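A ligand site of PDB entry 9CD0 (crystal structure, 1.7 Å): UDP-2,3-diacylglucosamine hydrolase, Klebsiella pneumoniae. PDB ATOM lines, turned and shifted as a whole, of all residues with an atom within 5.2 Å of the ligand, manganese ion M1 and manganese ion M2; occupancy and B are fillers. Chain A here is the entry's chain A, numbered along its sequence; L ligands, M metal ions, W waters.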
ATOM      1  N   ASP A   8      18.363  -5.374   1.966  1.00  0.00           N
ATOM      2  CA  ASP A   8      18.027  -5.657   3.325  1.00  0.00           C
ATOM      3  C   ASP A   8      16.572  -6.113   3.503  1.00  0.00           C
ATOM      4  O   ASP A   8      15.916  -5.794   4.508  1.00  0.00           O
ATOM      5  CB  ASP A   8      18.344  -4.427   4.173  1.00  0.00           C
ATOM      6  CG  ASP A   8      19.847  -4.102   4.080  1.00  0.00           C
ATOM      7  OD1 ASP A   8      20.597  -4.959   4.540  1.00  0.00           O
ATOM      8  OD2 ASP A   8      20.244  -3.066   3.506  1.00  0.00           O
ATOM      9  N   HIS A  10      16.141  -9.378   3.924  1.00  0.00           N
ATOM     10  CA  HIS A  10      16.396 -10.438   4.909  1.00  0.00           C
ATOM     11  C   HIS A  10      15.295 -11.501   4.854  1.00  0.00           C
ATOM     12  O   HIS A  10      14.725 -11.902   5.882  1.00  0.00           O
ATOM     13  CB  HIS A  10      16.546  -9.846   6.342  1.00  0.00           C
ATOM     14  CG  HIS A  10      17.798  -9.028   6.548  1.00  0.00           C
ATOM     15  ND1 HIS A  10      18.954  -9.554   7.090  1.00  0.00           N
ATOM     16  CD2 HIS A  10      18.110  -7.770   6.163  1.00  0.00           C
ATOM     17  CE1 HIS A  10      19.890  -8.613   7.112  1.00  0.00           C
ATOM     18  NE2 HIS A  10      19.399  -7.522   6.565  1.00  0.00           N
ATOM     19  N   ASP A  41      21.777  -8.600   1.075  1.00  0.00           N
ATOM     20  CA  ASP A  41      20.858  -9.042   2.130  1.00  0.00           C
ATOM     21  C   ASP A  41      19.429  -9.197   1.590  1.00  0.00           C
ATOM     22  O   ASP A  41      18.430  -8.834   2.237  1.00  0.00           O
ATOM     23  CB  ASP A  41      20.899  -8.121   3.369  1.00  0.00           C
ATOM     24  CG  ASP A  41      22.242  -8.174   4.102  1.00  0.00           C
ATOM     25  OD1 ASP A  41      23.142  -8.974   3.701  1.00  0.00           O
ATOM     26  OD2 ASP A  41      22.340  -7.375   5.050  1.00  0.00           O
ATOM     27  N   GLU A  44      17.981 -13.640   4.513  1.00  0.00           N
ATOM     28  CA  GLU A  44      18.539 -13.656   5.856  1.00  0.00           C
ATOM     29  C   GLU A  44      19.761 -14.575   5.971  1.00  0.00           C
ATOM     30  O   GLU A  44      20.633 -14.350   6.824  1.00  0.00           O
ATOM     31  CB  GLU A  44      17.447 -14.098   6.843  1.00  0.00           C
ATOM     32  CG  GLU A  44      17.974 -14.276   8.313  1.00  0.00           C
ATOM     33  CD  GLU A  44      18.453 -13.032   9.010  1.00  0.00           C
ATOM     34  OE1 GLU A  44      18.307 -11.920   8.479  1.00  0.00           O
ATOM     35  OE2 GLU A  44      18.969 -13.164  10.133  1.00  0.00           O
ATOM     36  N   ALA A  45      19.820 -15.645   5.161  1.00  0.00           N
ATOM     37  CA  ALA A  45      20.958 -16.537   5.203  1.00  0.00           C
ATOM     38  C   ALA A  45      21.115 -17.201   3.831  1.00  0.00           C
ATOM     39  O   ALA A  45      20.166 -17.276   3.061  1.00  0.00           O
ATOM     40  CB  ALA A  45      20.758 -17.610   6.261  1.00  0.00           C
ATOM     41  N   TRP A  46      22.318 -17.699   3.554  1.00  0.00           N
ATOM     42  CA  TRP A  46      22.537 -18.495   2.340  1.00  0.00           C
ATOM     43  C   TRP A  46      23.685 -19.442   2.587  1.00  0.00           C
ATOM     44  O   TRP A  46      24.735 -19.000   3.048  1.00  0.00           O
ATOM     45  CB  TRP A  46      22.880 -17.610   1.143  1.00  0.00           C
ATOM     46  CG  TRP A  46      22.646 -18.243  -0.210  1.00  0.00           C
ATOM     47  CD1 TRP A  46      23.563 -18.871  -0.994  1.00  0.00           C
ATOM     48  CD2 TRP A  46      21.387 -18.283  -0.919  1.00  0.00           C
ATOM     49  NE1 TRP A  46      22.939 -19.303  -2.186  1.00  0.00           N
ATOM     50  CE2 TRP A  46      21.622 -18.949  -2.149  1.00  0.00           C
ATOM     51  CE3 TRP A  46      20.093 -17.816  -0.619  1.00  0.00           C
ATOM     52  CZ2 TRP A  46      20.602 -19.105  -3.104  1.00  0.00           C
ATOM     53  CZ3 TRP A  46      19.063 -17.959  -1.618  1.00  0.00           C
ATOM     54  CH2 TRP A  46      19.342 -18.606  -2.819  1.00  0.00           C
ATOM     55  N   ILE A  47      23.484 -20.712   2.249  1.00  0.00           N
ATOM     56  CA  ILE A  47      24.531 -21.691   2.471  1.00  0.00           C
ATOM     57  C   ILE A  47      24.961 -22.345   1.168  1.00  0.00           C
ATOM     58  O   ILE A  47      25.711 -23.315   1.190  1.00  0.00           O
ATOM     59  CB  ILE A  47      24.113 -22.767   3.505  1.00  0.00           C
ATOM     60  CG1 ILE A  47      22.839 -23.504   3.082  1.00  0.00           C
ATOM     61  CG2 ILE A  47      23.930 -22.176   4.928  1.00  0.00           C
ATOM     62  CD1 ILE A  47      22.596 -24.773   3.866  1.00  0.00           C
ATOM     63  N   GLY A  78      25.275  -9.147   0.032  1.00  0.00           N
ATOM     64  CA  GLY A  78      25.321  -8.598   1.382  1.00  0.00           C
ATOM     65  C   GLY A  78      26.204  -9.450   2.298  1.00  0.00           C
ATOM     66  O   GLY A  78      26.790 -10.435   1.904  1.00  0.00           O
ATOM     67  N   ASN A  79      26.279  -9.035   3.571  1.00  0.00           N
ATOM     68  CA  ASN A  79      26.964  -9.876   4.562  1.00  0.00           C
ATOM     69  C   ASN A  79      26.183 -11.149   4.883  1.00  0.00           C
ATOM     70  O   ASN A  79      26.783 -12.123   5.366  1.00  0.00           O
ATOM     71  CB  ASN A  79      27.231  -9.045   5.816  1.00  0.00           C
ATOM     72  CG  ASN A  79      25.961  -8.536   6.466  1.00  0.00           C
ATOM     73  OD1 ASN A  79      25.311  -7.698   5.901  1.00  0.00           O
ATOM     74  ND2 ASN A  79      25.642  -9.019   7.650  1.00  0.00           N
ATOM     75  N   ARG A  80      24.867 -11.149   4.670  1.00  0.00           N
ATOM     76  CA  ARG A  80      24.099 -12.360   4.954  1.00  0.00           C
ATOM     77  C   ARG A  80      24.209 -13.367   3.800  1.00  0.00           C
ATOM     78  O   ARG A  80      24.320 -14.579   4.056  1.00  0.00           O
ATOM     79  CB  ARG A  80      22.622 -12.063   5.238  1.00  0.00           C
ATOM     80  CG  ARG A  80      22.408 -11.042   6.338  1.00  0.00           C
ATOM     81  CD  ARG A  80      23.054 -11.483   7.655  1.00  0.00           C
ATOM     82  NE  ARG A  80      22.484 -12.740   8.131  1.00  0.00           N
ATOM     83  CZ  ARG A  80      22.595 -13.192   9.380  1.00  0.00           C
ATOM     84  NH1 ARG A  80      23.322 -12.578  10.292  1.00  0.00           N
ATOM     85  NH2 ARG A  80      21.944 -14.302   9.728  1.00  0.00           N
ATOM     86  N   PHE A  82      26.357 -13.653   0.928  1.00  0.00           N
ATOM     87  CA  PHE A  82      27.562 -13.601   0.093  1.00  0.00           C
ATOM     88  C   PHE A  82      27.796 -14.923  -0.670  1.00  0.00           C
ATOM     89  O   PHE A  82      28.630 -14.966  -1.591  1.00  0.00           O
ATOM     90  CB  PHE A  82      28.803 -13.275   0.960  1.00  0.00           C
ATOM     91  CG  PHE A  82      29.029 -14.227   2.134  1.00  0.00           C
ATOM     92  CD1 PHE A  82      29.759 -15.407   1.997  1.00  0.00           C
ATOM     93  CD2 PHE A  82      28.522 -13.922   3.408  1.00  0.00           C
ATOM     94  CE1 PHE A  82      29.921 -16.258   3.089  1.00  0.00           C
ATOM     95  CE2 PHE A  82      28.737 -14.765   4.488  1.00  0.00           C
ATOM     96  CZ  PHE A  82      29.383 -15.956   4.302  1.00  0.00           C
ATOM     97  N   LEU A  83      27.141 -16.004  -0.271  1.00  0.00           N
ATOM     98  CA  LEU A  83      27.310 -17.240  -1.037  1.00  0.00           C
ATOM     99  C   LEU A  83      26.350 -17.399  -2.218  1.00  0.00           C
ATOM    100  O   LEU A  83      26.400 -18.438  -2.879  1.00  0.00           O
ATOM    101  CB  LEU A  83      27.184 -18.461  -0.115  1.00  0.00           C
ATOM    102  CG  LEU A  83      28.339 -18.577   0.911  1.00  0.00           C
ATOM    103  CD1 LEU A  83      28.161 -19.797   1.865  1.00  0.00           C
ATOM    104  CD2 LEU A  83      29.759 -18.641   0.277  1.00  0.00           C
ATOM    105  N   HIS A 114      26.788  -2.786  -1.034  1.00  0.00           N
ATOM    106  CA  HIS A 114      25.915  -3.160   0.082  1.00  0.00           C
ATOM    107  C   HIS A 114      26.075  -2.170   1.242  1.00  0.00           C
ATOM    108  O   HIS A 114      25.080  -1.792   1.863  1.00  0.00           O
ATOM    109  CB  HIS A 114      26.211  -4.585   0.594  1.00  0.00           C
ATOM    110  CG  HIS A 114      25.326  -4.984   1.722  1.00  0.00           C
ATOM    111  ND1 HIS A 114      23.949  -5.050   1.617  1.00  0.00           N
ATOM    112  CD2 HIS A 114      25.639  -5.322   2.999  1.00  0.00           C
ATOM    113  CE1 HIS A 114      23.455  -5.436   2.804  1.00  0.00           C
ATOM    114  NE2 HIS A 114      24.462  -5.594   3.653  1.00  0.00           N
ATOM    115  N   ASP A 122      33.949  -1.543  12.794  1.00  0.00           N
ATOM    116  CA  ASP A 122      33.545  -2.833  13.353  1.00  0.00           C
ATOM    117  C   ASP A 122      34.594  -3.870  12.949  1.00  0.00           C
ATOM    118  O   ASP A 122      34.435  -4.664  12.022  1.00  0.00           O
ATOM    119  CB  ASP A 122      32.147  -3.266  12.897  1.00  0.00           C
ATOM    120  CG  ASP A 122      31.628  -4.446  13.752  1.00  0.00           C
ATOM    121  OD1 ASP A 122      32.474  -5.189  14.333  1.00  0.00           O
ATOM    122  OD2 ASP A 122      30.428  -4.607  13.885  1.00  0.00           O
ATOM    123  N   GLY A 124      35.467  -6.547  14.416  1.00  0.00           N
ATOM    124  CA  GLY A 124      35.074  -7.944  14.539  1.00  0.00           C
ATOM    125  C   GLY A 124      34.261  -8.394  13.341  1.00  0.00           C
ATOM    126  O   GLY A 124      34.457  -9.507  12.828  1.00  0.00           O
ATOM    127  N   TYR A 125      33.366  -7.525  12.840  1.00  0.00           N
ATOM    128  CA  TYR A 125      32.687  -7.845  11.580  1.00  0.00           C
ATOM    129  C   TYR A 125      33.706  -7.969  10.450  1.00  0.00           C
ATOM    130  O   TYR A 125      33.620  -8.873   9.633  1.00  0.00           O
ATOM    131  CB  TYR A 125      31.630  -6.764  11.214  1.00  0.00           C
ATOM    132  CG  TYR A 125      31.177  -7.038   9.811  1.00  0.00           C
ATOM    133  CD1 TYR A 125      30.564  -8.228   9.525  1.00  0.00           C
ATOM    134  CD2 TYR A 125      31.523  -6.193   8.747  1.00  0.00           C
ATOM    135  CE1 TYR A 125      30.205  -8.593   8.232  1.00  0.00           C
ATOM    136  CE2 TYR A 125      31.169  -6.516   7.436  1.00  0.00           C
ATOM    137  CZ  TYR A 125      30.508  -7.732   7.198  1.00  0.00           C
ATOM    138  OH  TYR A 125      30.161  -8.127   5.931  1.00  0.00           O
ATOM    139  N   PHE A 128      35.421 -11.348  10.552  1.00  0.00           N
ATOM    140  CA  PHE A 128      34.499 -12.338   9.972  1.00  0.00           C
ATOM    141  C   PHE A 128      34.437 -12.219   8.442  1.00  0.00           C
ATOM    142  O   PHE A 128      34.510 -13.226   7.717  1.00  0.00           O
ATOM    143  CB  PHE A 128      33.125 -12.151  10.630  1.00  0.00           C
ATOM    144  CG  PHE A 128      31.989 -12.934   9.991  1.00  0.00           C
ATOM    145  CD1 PHE A 128      31.293 -12.426   8.878  1.00  0.00           C
ATOM    146  CD2 PHE A 128      31.594 -14.159  10.528  1.00  0.00           C
ATOM    147  CE1 PHE A 128      30.255 -13.138   8.306  1.00  0.00           C
ATOM    148  CE2 PHE A 128      30.557 -14.872   9.955  1.00  0.00           C
ATOM    149  CZ  PHE A 128      29.901 -14.375   8.825  1.00  0.00           C
ATOM    150  N   LYS A 131      37.347 -13.603   6.591  1.00  0.00           N
ATOM    151  CA  LYS A 131      37.397 -15.070   6.621  1.00  0.00           C
ATOM    152  C   LYS A 131      36.410 -15.668   5.630  1.00  0.00           C
ATOM    153  O   LYS A 131      36.781 -16.517   4.817  1.00  0.00           O
ATOM    154  CB  LYS A 131      37.148 -15.578   8.049  1.00  0.00           C
ATOM    155  CG  LYS A 131      36.613 -16.982   8.197  1.00  0.00           C
ATOM    156  CD  LYS A 131      36.252 -17.254   9.644  1.00  0.00           C
ATOM    157  CE  LYS A 131      35.649 -18.637   9.807  1.00  0.00           C
ATOM    158  NZ  LYS A 131      36.598 -19.717   9.495  1.00  0.00           N
ATOM    159  N   VAL A 132      35.149 -15.209   5.630  1.00  0.00           N
ATOM    160  CA  VAL A 132      34.149 -15.863   4.780  1.00  0.00           C
ATOM    161  C   VAL A 132      34.206 -15.413   3.333  1.00  0.00           C
ATOM    162  O   VAL A 132      33.551 -16.046   2.498  1.00  0.00           O
ATOM    163  CB  VAL A 132      32.703 -15.700   5.282  1.00  0.00           C
ATOM    164  CG1 VAL A 132      32.497 -16.389   6.642  1.00  0.00           C
ATOM    165  CG2 VAL A 132      32.259 -14.167   5.275  1.00  0.00           C
ATOM    166  N   ILE A 137      38.195 -20.862   1.841  1.00  0.00           N
ATOM    167  CA  ILE A 137      37.232 -21.090   2.901  1.00  0.00           C
ATOM    168  C   ILE A 137      35.821 -21.259   2.333  1.00  0.00           C
ATOM    169  O   ILE A 137      35.064 -22.104   2.799  1.00  0.00           O
ATOM    170  CB  ILE A 137      37.356 -19.946   3.927  1.00  0.00           C
ATOM    171  CG1 ILE A 137      38.777 -19.962   4.519  1.00  0.00           C
ATOM    172  CG2 ILE A 137      36.194 -20.034   4.950  1.00  0.00           C
ATOM    173  CD1 ILE A 137      38.961 -18.958   5.682  1.00  0.00           C
ATOM    174  N   GLN A 138      35.428 -20.457   1.323  1.00  0.00           N
ATOM    175  CA  GLN A 138      34.138 -20.675   0.670  1.00  0.00           C
ATOM    176  C   GLN A 138      34.085 -22.031   0.001  1.00  0.00           C
ATOM    177  O   GLN A 138      33.039 -22.718   0.039  1.00  0.00           O
ATOM    178  CB  GLN A 138      33.853 -19.585  -0.383  1.00  0.00           C
ATOM    179  CG  GLN A 138      33.764 -18.242   0.208  1.00  0.00           C
ATOM    180  CD  GLN A 138      33.289 -17.230  -0.797  1.00  0.00           C
ATOM    181  OE1 GLN A 138      33.182 -17.521  -1.985  1.00  0.00           O
ATOM    182  NE2 GLN A 138      32.910 -16.074  -0.321  1.00  0.00           N
ATOM    183  N   PHE A 141      33.643 -24.750   2.635  1.00  0.00           N
ATOM    184  CA  PHE A 141      32.307 -24.781   3.227  1.00  0.00           C
ATOM    185  C   PHE A 141      31.288 -25.366   2.246  1.00  0.00           C
ATOM    186  O   PHE A 141      30.450 -26.188   2.625  1.00  0.00           O
ATOM    187  CB  PHE A 141      31.871 -23.356   3.652  1.00  0.00           C
ATOM    188  CG  PHE A 141      30.466 -23.279   4.242  1.00  0.00           C
ATOM    189  CD1 PHE A 141      30.254 -23.593   5.558  1.00  0.00           C
ATOM    190  CD2 PHE A 141      29.371 -22.851   3.470  1.00  0.00           C
ATOM    191  CE1 PHE A 141      28.995 -23.500   6.113  1.00  0.00           C
ATOM    192  CE2 PHE A 141      28.116 -22.742   3.999  1.00  0.00           C
ATOM    193  CZ  PHE A 141      27.912 -23.065   5.343  1.00  0.00           C
ATOM    194  N   ILE A 152      25.833 -25.877  10.692  1.00  0.00           N
ATOM    195  CA  ILE A 152      26.823 -24.832  10.949  1.00  0.00           C
ATOM    196  C   ILE A 152      26.145 -23.460  10.979  1.00  0.00           C
ATOM    197  O   ILE A 152      26.349 -22.659  11.900  1.00  0.00           O
ATOM    198  CB  ILE A 152      27.916 -24.879   9.870  1.00  0.00           C
ATOM    199  CG1 ILE A 152      28.756 -26.174  10.027  1.00  0.00           C
ATOM    200  CG2 ILE A 152      28.818 -23.617  10.037  1.00  0.00           C
ATOM    201  CD1 ILE A 152      29.740 -26.392   8.845  1.00  0.00           C
ATOM    202  N   ALA A 153      25.353 -23.180   9.956  1.00  0.00           N
ATOM    203  CA  ALA A 153      24.730 -21.850   9.845  1.00  0.00           C
ATOM    204  C   ALA A 153      23.771 -21.583  11.005  1.00  0.00           C
ATOM    205  O   ALA A 153      23.720 -20.464  11.546  1.00  0.00           O
ATOM    206  CB  ALA A 153      24.005 -21.709   8.508  1.00  0.00           C
ATOM    207  N   MET A 156      25.795 -20.742  14.019  1.00  0.00           N
ATOM    208  CA  MET A 156      26.510 -19.471  13.917  1.00  0.00           C
ATOM    209  C   MET A 156      25.531 -18.314  14.101  1.00  0.00           C
ATOM    210  O   MET A 156      25.843 -17.290  14.725  1.00  0.00           O
ATOM    211  CB  MET A 156      27.107 -19.466  12.528  1.00  0.00           C
ATOM    212  CG  MET A 156      28.450 -20.215  12.523  1.00  0.00           C
ATOM    213  SD  MET A 156      29.402 -20.093  10.998  1.00  0.00           S
ATOM    214  CE  MET A 156      29.812 -18.331  11.013  1.00  0.00           C
ATOM    215  N   ARG A 157      24.334 -18.449  13.525  1.00  0.00           N
ATOM    216  CA  ARG A 157      23.272 -17.464  13.781  1.00  0.00           C
ATOM    217  C   ARG A 157      22.891 -17.400  15.275  1.00  0.00           C
ATOM    218  O   ARG A 157      22.754 -16.308  15.846  1.00  0.00           O
ATOM    219  CB  ARG A 157      22.064 -17.789  12.907  1.00  0.00           C
ATOM    220  CG  ARG A 157      22.383 -17.576  11.389  1.00  0.00           C
ATOM    221  CD  ARG A 157      21.108 -17.597  10.596  1.00  0.00           C
ATOM    222  NE  ARG A 157      20.426 -18.877  10.725  1.00  0.00           N
ATOM    223  CZ  ARG A 157      20.556 -19.891   9.888  1.00  0.00           C
ATOM    224  NH1 ARG A 157      21.366 -19.802   8.827  1.00  0.00           N
ATOM    225  NH2 ARG A 157      19.855 -21.009  10.096  1.00  0.00           N
ATOM    226  N   SER A 160      25.594 -15.575  17.047  1.00  0.00           N
ATOM    227  CA  SER A 160      25.635 -14.146  16.756  1.00  0.00           C
ATOM    228  C   SER A 160      24.537 -13.426  17.536  1.00  0.00           C
ATOM    229  O   SER A 160      24.776 -12.357  18.121  1.00  0.00           O
ATOM    230  CB  SER A 160      25.505 -13.910  15.244  1.00  0.00           C
ATOM    231  OG  SER A 160      25.095 -12.581  14.947  1.00  0.00           O
ATOM    232  N   GLU A 170      21.840  -4.879  16.480  1.00  0.00           N
ATOM    233  CA  GLU A 170      22.689  -3.686  16.441  1.00  0.00           C
ATOM    234  C   GLU A 170      23.801  -3.808  15.387  1.00  0.00           C
ATOM    235  O   GLU A 170      24.799  -4.496  15.607  1.00  0.00           O
ATOM    236  CB  GLU A 170      23.282  -3.405  17.848  1.00  0.00           C
ATOM    237  N   ILE A 171      23.597  -3.147  14.245  1.00  0.00           N
ATOM    238  CA  ILE A 171      24.555  -3.077  13.145  1.00  0.00           C
ATOM    239  C   ILE A 171      25.313  -1.771  13.262  1.00  0.00           C
ATOM    240  O   ILE A 171      24.706  -0.706  13.440  1.00  0.00           O
ATOM    241  CB  ILE A 171      23.841  -3.173  11.784  1.00  0.00           C
ATOM    242  CG1 ILE A 171      23.030  -4.492  11.694  1.00  0.00           C
ATOM    243  CG2 ILE A 171      24.780  -2.924  10.629  1.00  0.00           C
ATOM    244  CD1 ILE A 171      22.040  -4.521  10.553  1.00  0.00           C
ATOM    245  N   HIS A 195      22.696  -2.132   4.150  1.00  0.00           N
ATOM    246  CA  HIS A 195      23.388  -2.693   5.314  1.00  0.00           C
ATOM    247  C   HIS A 195      23.106  -2.065   6.679  1.00  0.00           C
ATOM    248  O   HIS A 195      22.850  -2.808   7.633  1.00  0.00           O
ATOM    249  CB  HIS A 195      24.903  -2.715   5.094  1.00  0.00           C
ATOM    250  CG  HIS A 195      25.650  -3.394   6.222  1.00  0.00           C
ATOM    251  ND1 HIS A 195      25.518  -4.740   6.474  1.00  0.00           N
ATOM    252  CD2 HIS A 195      26.460  -2.915   7.200  1.00  0.00           C
ATOM    253  CE1 HIS A 195      26.244  -5.071   7.531  1.00  0.00           C
ATOM    254  NE2 HIS A 195      26.842  -3.987   7.978  1.00  0.00           N
ATOM    255  N   HIS A 197      20.625  -0.186   7.757  1.00  0.00           N
ATOM    256  CA  HIS A 197      19.213  -0.209   8.161  1.00  0.00           C
ATOM    257  C   HIS A 197      18.784   1.155   8.719  1.00  0.00           C
ATOM    258  O   HIS A 197      17.927   1.250   9.619  1.00  0.00           O
ATOM    259  CB  HIS A 197      18.939  -1.331   9.176  1.00  0.00           C
ATOM    260  CG  HIS A 197      19.171  -2.733   8.631  1.00  0.00           C
ATOM    261  ND1 HIS A 197      18.848  -3.876   9.352  1.00  0.00           N
ATOM    262  CD2 HIS A 197      19.664  -3.160   7.447  1.00  0.00           C
ATOM    263  CE1 HIS A 197      19.173  -4.942   8.633  1.00  0.00           C
ATOM    264  NE2 HIS A 197      19.665  -4.530   7.483  1.00  0.00           N
HETATM  265  C1  LIG L   1      27.492 -20.101   7.693  1.00  0.00           C
HETATM  266  C2  LIG L   1      25.385 -16.116   9.500  1.00  0.00           C
HETATM  267  C3  LIG L   1      26.365 -13.919   9.439  1.00  0.00           C
HETATM  268  C4  LIG L   1      27.308 -11.638   9.994  1.00  0.00           C
HETATM  269  C5  LIG L   1      29.259 -11.443  11.497  1.00  0.00           C
HETATM  270  C6  LIG L   1      29.580  -9.570  12.941  1.00  0.00           C
HETATM  271  C7  LIG L   1      27.635  -9.622  11.529  1.00  0.00           C
HETATM  272  C8  LIG L   1      31.578 -19.791   5.130  1.00  0.00           C
HETATM  273  C9  LIG L   1      29.737 -19.948   6.457  1.00  0.00           C
HETATM  274  C10 LIG L   1      27.674 -19.043   5.424  1.00  0.00           C
HETATM  275  C11 LIG L   1      26.776 -17.921   5.934  1.00  0.00           C
HETATM  276  C12 LIG L   1      26.610 -18.934   8.149  1.00  0.00           C
HETATM  277  C13 LIG L   1      25.246 -16.008   8.119  1.00  0.00           C
HETATM  278  C14 LIG L   1      25.978 -15.044  10.161  1.00  0.00           C
HETATM  279  C15 LIG L   1      26.283 -13.807   8.034  1.00  0.00           C
HETATM  280  C16 LIG L   1      25.698 -14.896   7.379  1.00  0.00           C
HETATM  281  C17 LIG L   1      28.039 -10.861  11.051  1.00  0.00           C
HETATM  282  C18 LIG L   1      30.030 -10.789  12.462  1.00  0.00           C
HETATM  283  C19 LIG L   1      28.392  -9.002  12.485  1.00  0.00           C
HETATM  284  C20 LIG L   1      24.777  -8.779  13.398  1.00  0.00           C
HETATM  285  C21 LIG L   1      26.513  -7.563  10.643  1.00  0.00           C
HETATM  286  C22 LIG L   1      27.198 -13.647  11.651  1.00  0.00           C
HETATM  287  C23 LIG L   1      26.237 -14.795  11.633  1.00  0.00           C
HETATM  288  C24 LIG L   1      30.424 -20.628   7.502  1.00  0.00           C
HETATM  289  C25 LIG L   1      31.725 -20.865   7.246  1.00  0.00           C
HETATM  290  C26 LIG L   1      32.368 -20.449   6.082  1.00  0.00           C
HETATM  291  C27 LIG L   1      32.550 -21.594   8.333  1.00  0.00           C
HETATM  292  F1  LIG L   1      31.879 -22.545   8.844  1.00  0.00           F
HETATM  293  F2  LIG L   1      33.663 -21.986   7.837  1.00  0.00           F
HETATM  294  F3  LIG L   1      32.781 -20.821   9.270  1.00  0.00           F
HETATM  295  N1  LIG L   1      30.310 -19.593   5.337  1.00  0.00           N
HETATM  296  N2  LIG L   1      28.364 -19.663   6.590  1.00  0.00           N
HETATM  297  N3  LIG L   1      25.894 -18.411   6.944  1.00  0.00           N
HETATM  298  N4  LIG L   1      26.968 -12.981  10.373  1.00  0.00           N
HETATM  299  N5  LIG L   1      26.437  -8.953  11.133  1.00  0.00           N
HETATM  300  O1  LIG L   1      23.769 -18.078   8.213  1.00  0.00           O
HETATM  301  O2  LIG L   1      23.998 -17.099   6.077  1.00  0.00           O
HETATM  302  O3  LIG L   1      27.074 -11.159   8.926  1.00  0.00           O
HETATM  303  O4  LIG L   1      23.923  -9.180  10.853  1.00  0.00           O
HETATM  304  O5  LIG L   1      25.071 -10.970  11.922  1.00  0.00           O
HETATM  305  S1  LIG L   1      24.562 -17.455   7.318  1.00  0.00           S
HETATM  306  S2  LIG L   1      25.014  -9.522  11.759  1.00  0.00           S
HETATM  307 CL1  LIG L   1      32.290 -19.264   3.605  1.00  0.00          CL
HETATM  308 MN    MN M   1      24.004  -6.196   5.679  1.00  0.00          MN
HETATM  309 MN    MN M   2      20.781  -5.961   6.261  1.00  0.00          MN
HETATM  310  O   HOH W   1      22.623  -5.714   7.011  1.00  0.00           O
HETATM  311  O   HOH W   2      20.859  -7.873  10.063  1.00  0.00           O
HETATM  312  O   HOH W   3      26.457  -5.987  14.292  1.00  0.00           O
HETATM  313  O   HOH W   4      23.041  -7.798   8.553  1.00  0.00           O
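Manganese ion M2 is bound by the side-chain carboxylate of Asp 8 (2.0 Å), water W1 (2.0 Å), a ring nitrogen (NE2) of His 10 (2.1 Å), a ring nitrogen (NE2) of His 197 (2.2 Å) and the side-chain carboxylate of Asp 41 (2.4 Å). Manganese ion M2 has five donor atoms within binding distance.
Merely in contact with the ligand: Ala 45 (3.2 Å), Ile 152 (3.5 Å), Phe 128 (3.5 Å), Phe 141 (3.5 Å), Val 132 (3.6 Å), Lys 131 (3.6 Å), Phe 82 (3.6 Å), Ala 153 (3.7 Å), Leu 83 (3.7 Å), Met 156 (3.7 Å), Gln 138 (3.7 Å) and Tyr 125 (3.8 Å). Hydrophobic or aromatic side chains within 4 Å of the ligand: Ala 45, Phe 82, Leu 83, Tyr 125, Phe 128, Val 132, Phe 141, Ile 152, Ala 153, Met 156 and His 195. 18 residues have an atom within 4 Å of the ligand: Ala 45, Trp 46, Asn 79, Arg 80, Phe 82, Leu 83, Tyr 125, Phe 128, Lys 131, Val 132, Gln 138, Phe 141, Ile 152, Ala 153, Met 156, Arg 157, Ser 160 and His 195. The nearest printed residue that does not touch the ligand is Ile 137 (4.01 Å).
Water W4 bridges an oxygen (O4) of the ligand (2.8 Å) and the side-chain amide nitrogen of Asn 79 (3.0 Å).
The side-chain amide nitrogen (ND2) of Asn 79 is in hydrogen-bond range of an oxygen (O3) of the ligand, at 2.9 Å. NH1 of Arg 80 lies within hydrogen-bond range of O5 of the ligand, at 2.9 Å. An oxygen (O1) of the ligand sits at hydrogen-bond distance from the guanidinium group (NH1) of Arg 157 (3.0 Å). The backbone NH (N) of Trp 46 is in hydrogen-bond range of an oxygen (O2) of the ligand. O5 of the ligand lies within hydrogen-bond range of OG of Ser 160 (3.4 Å).
The backbone NH (N) of His 195 lies within hydrogen-bond range of the side-chain carboxylate (OD2) of Asp 8 (2.7 Å). A ring nitrogen (ND1) of His 10 is in hydrogen-bond range of the side-chain carboxylate (OE1) of Glu 44 (2.8 Å). OD1 of Asp 41 lies within hydrogen-bond range of N of Arg 80, 2.9 Å away. The side-chain carboxylate (OE2) of Glu 44 lies within salt-bridge range of the guanidinium group (NH2) of Arg 80, 3.2 Å away. O of Val 132 sits at hydrogen-bond distance from NE2 of Gln 138 (2.9 Å). The backbone NH (N) of Tyr 125 lies within hydrogen-bond range of the side-chain carboxylate (OD1) of Asp 122 (2.9 Å).
Of the 31 residues printed, 4 come within 4 Å of manganese ion M2.
Manganese ion M1 is bound by water W1 (2.0 Å), the side-chain amide oxygen (OD1) of Asn 79 (2.0 Å), the side-chain carboxylate (OD2) of Asp 41 (2.1 Å), a ring nitrogen (NE2) of His 114 (2.2 Å) and a ring nitrogen (ND1) of His 195 (2.2 Å). Manganese ion M1 has five donor atoms within binding distance.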
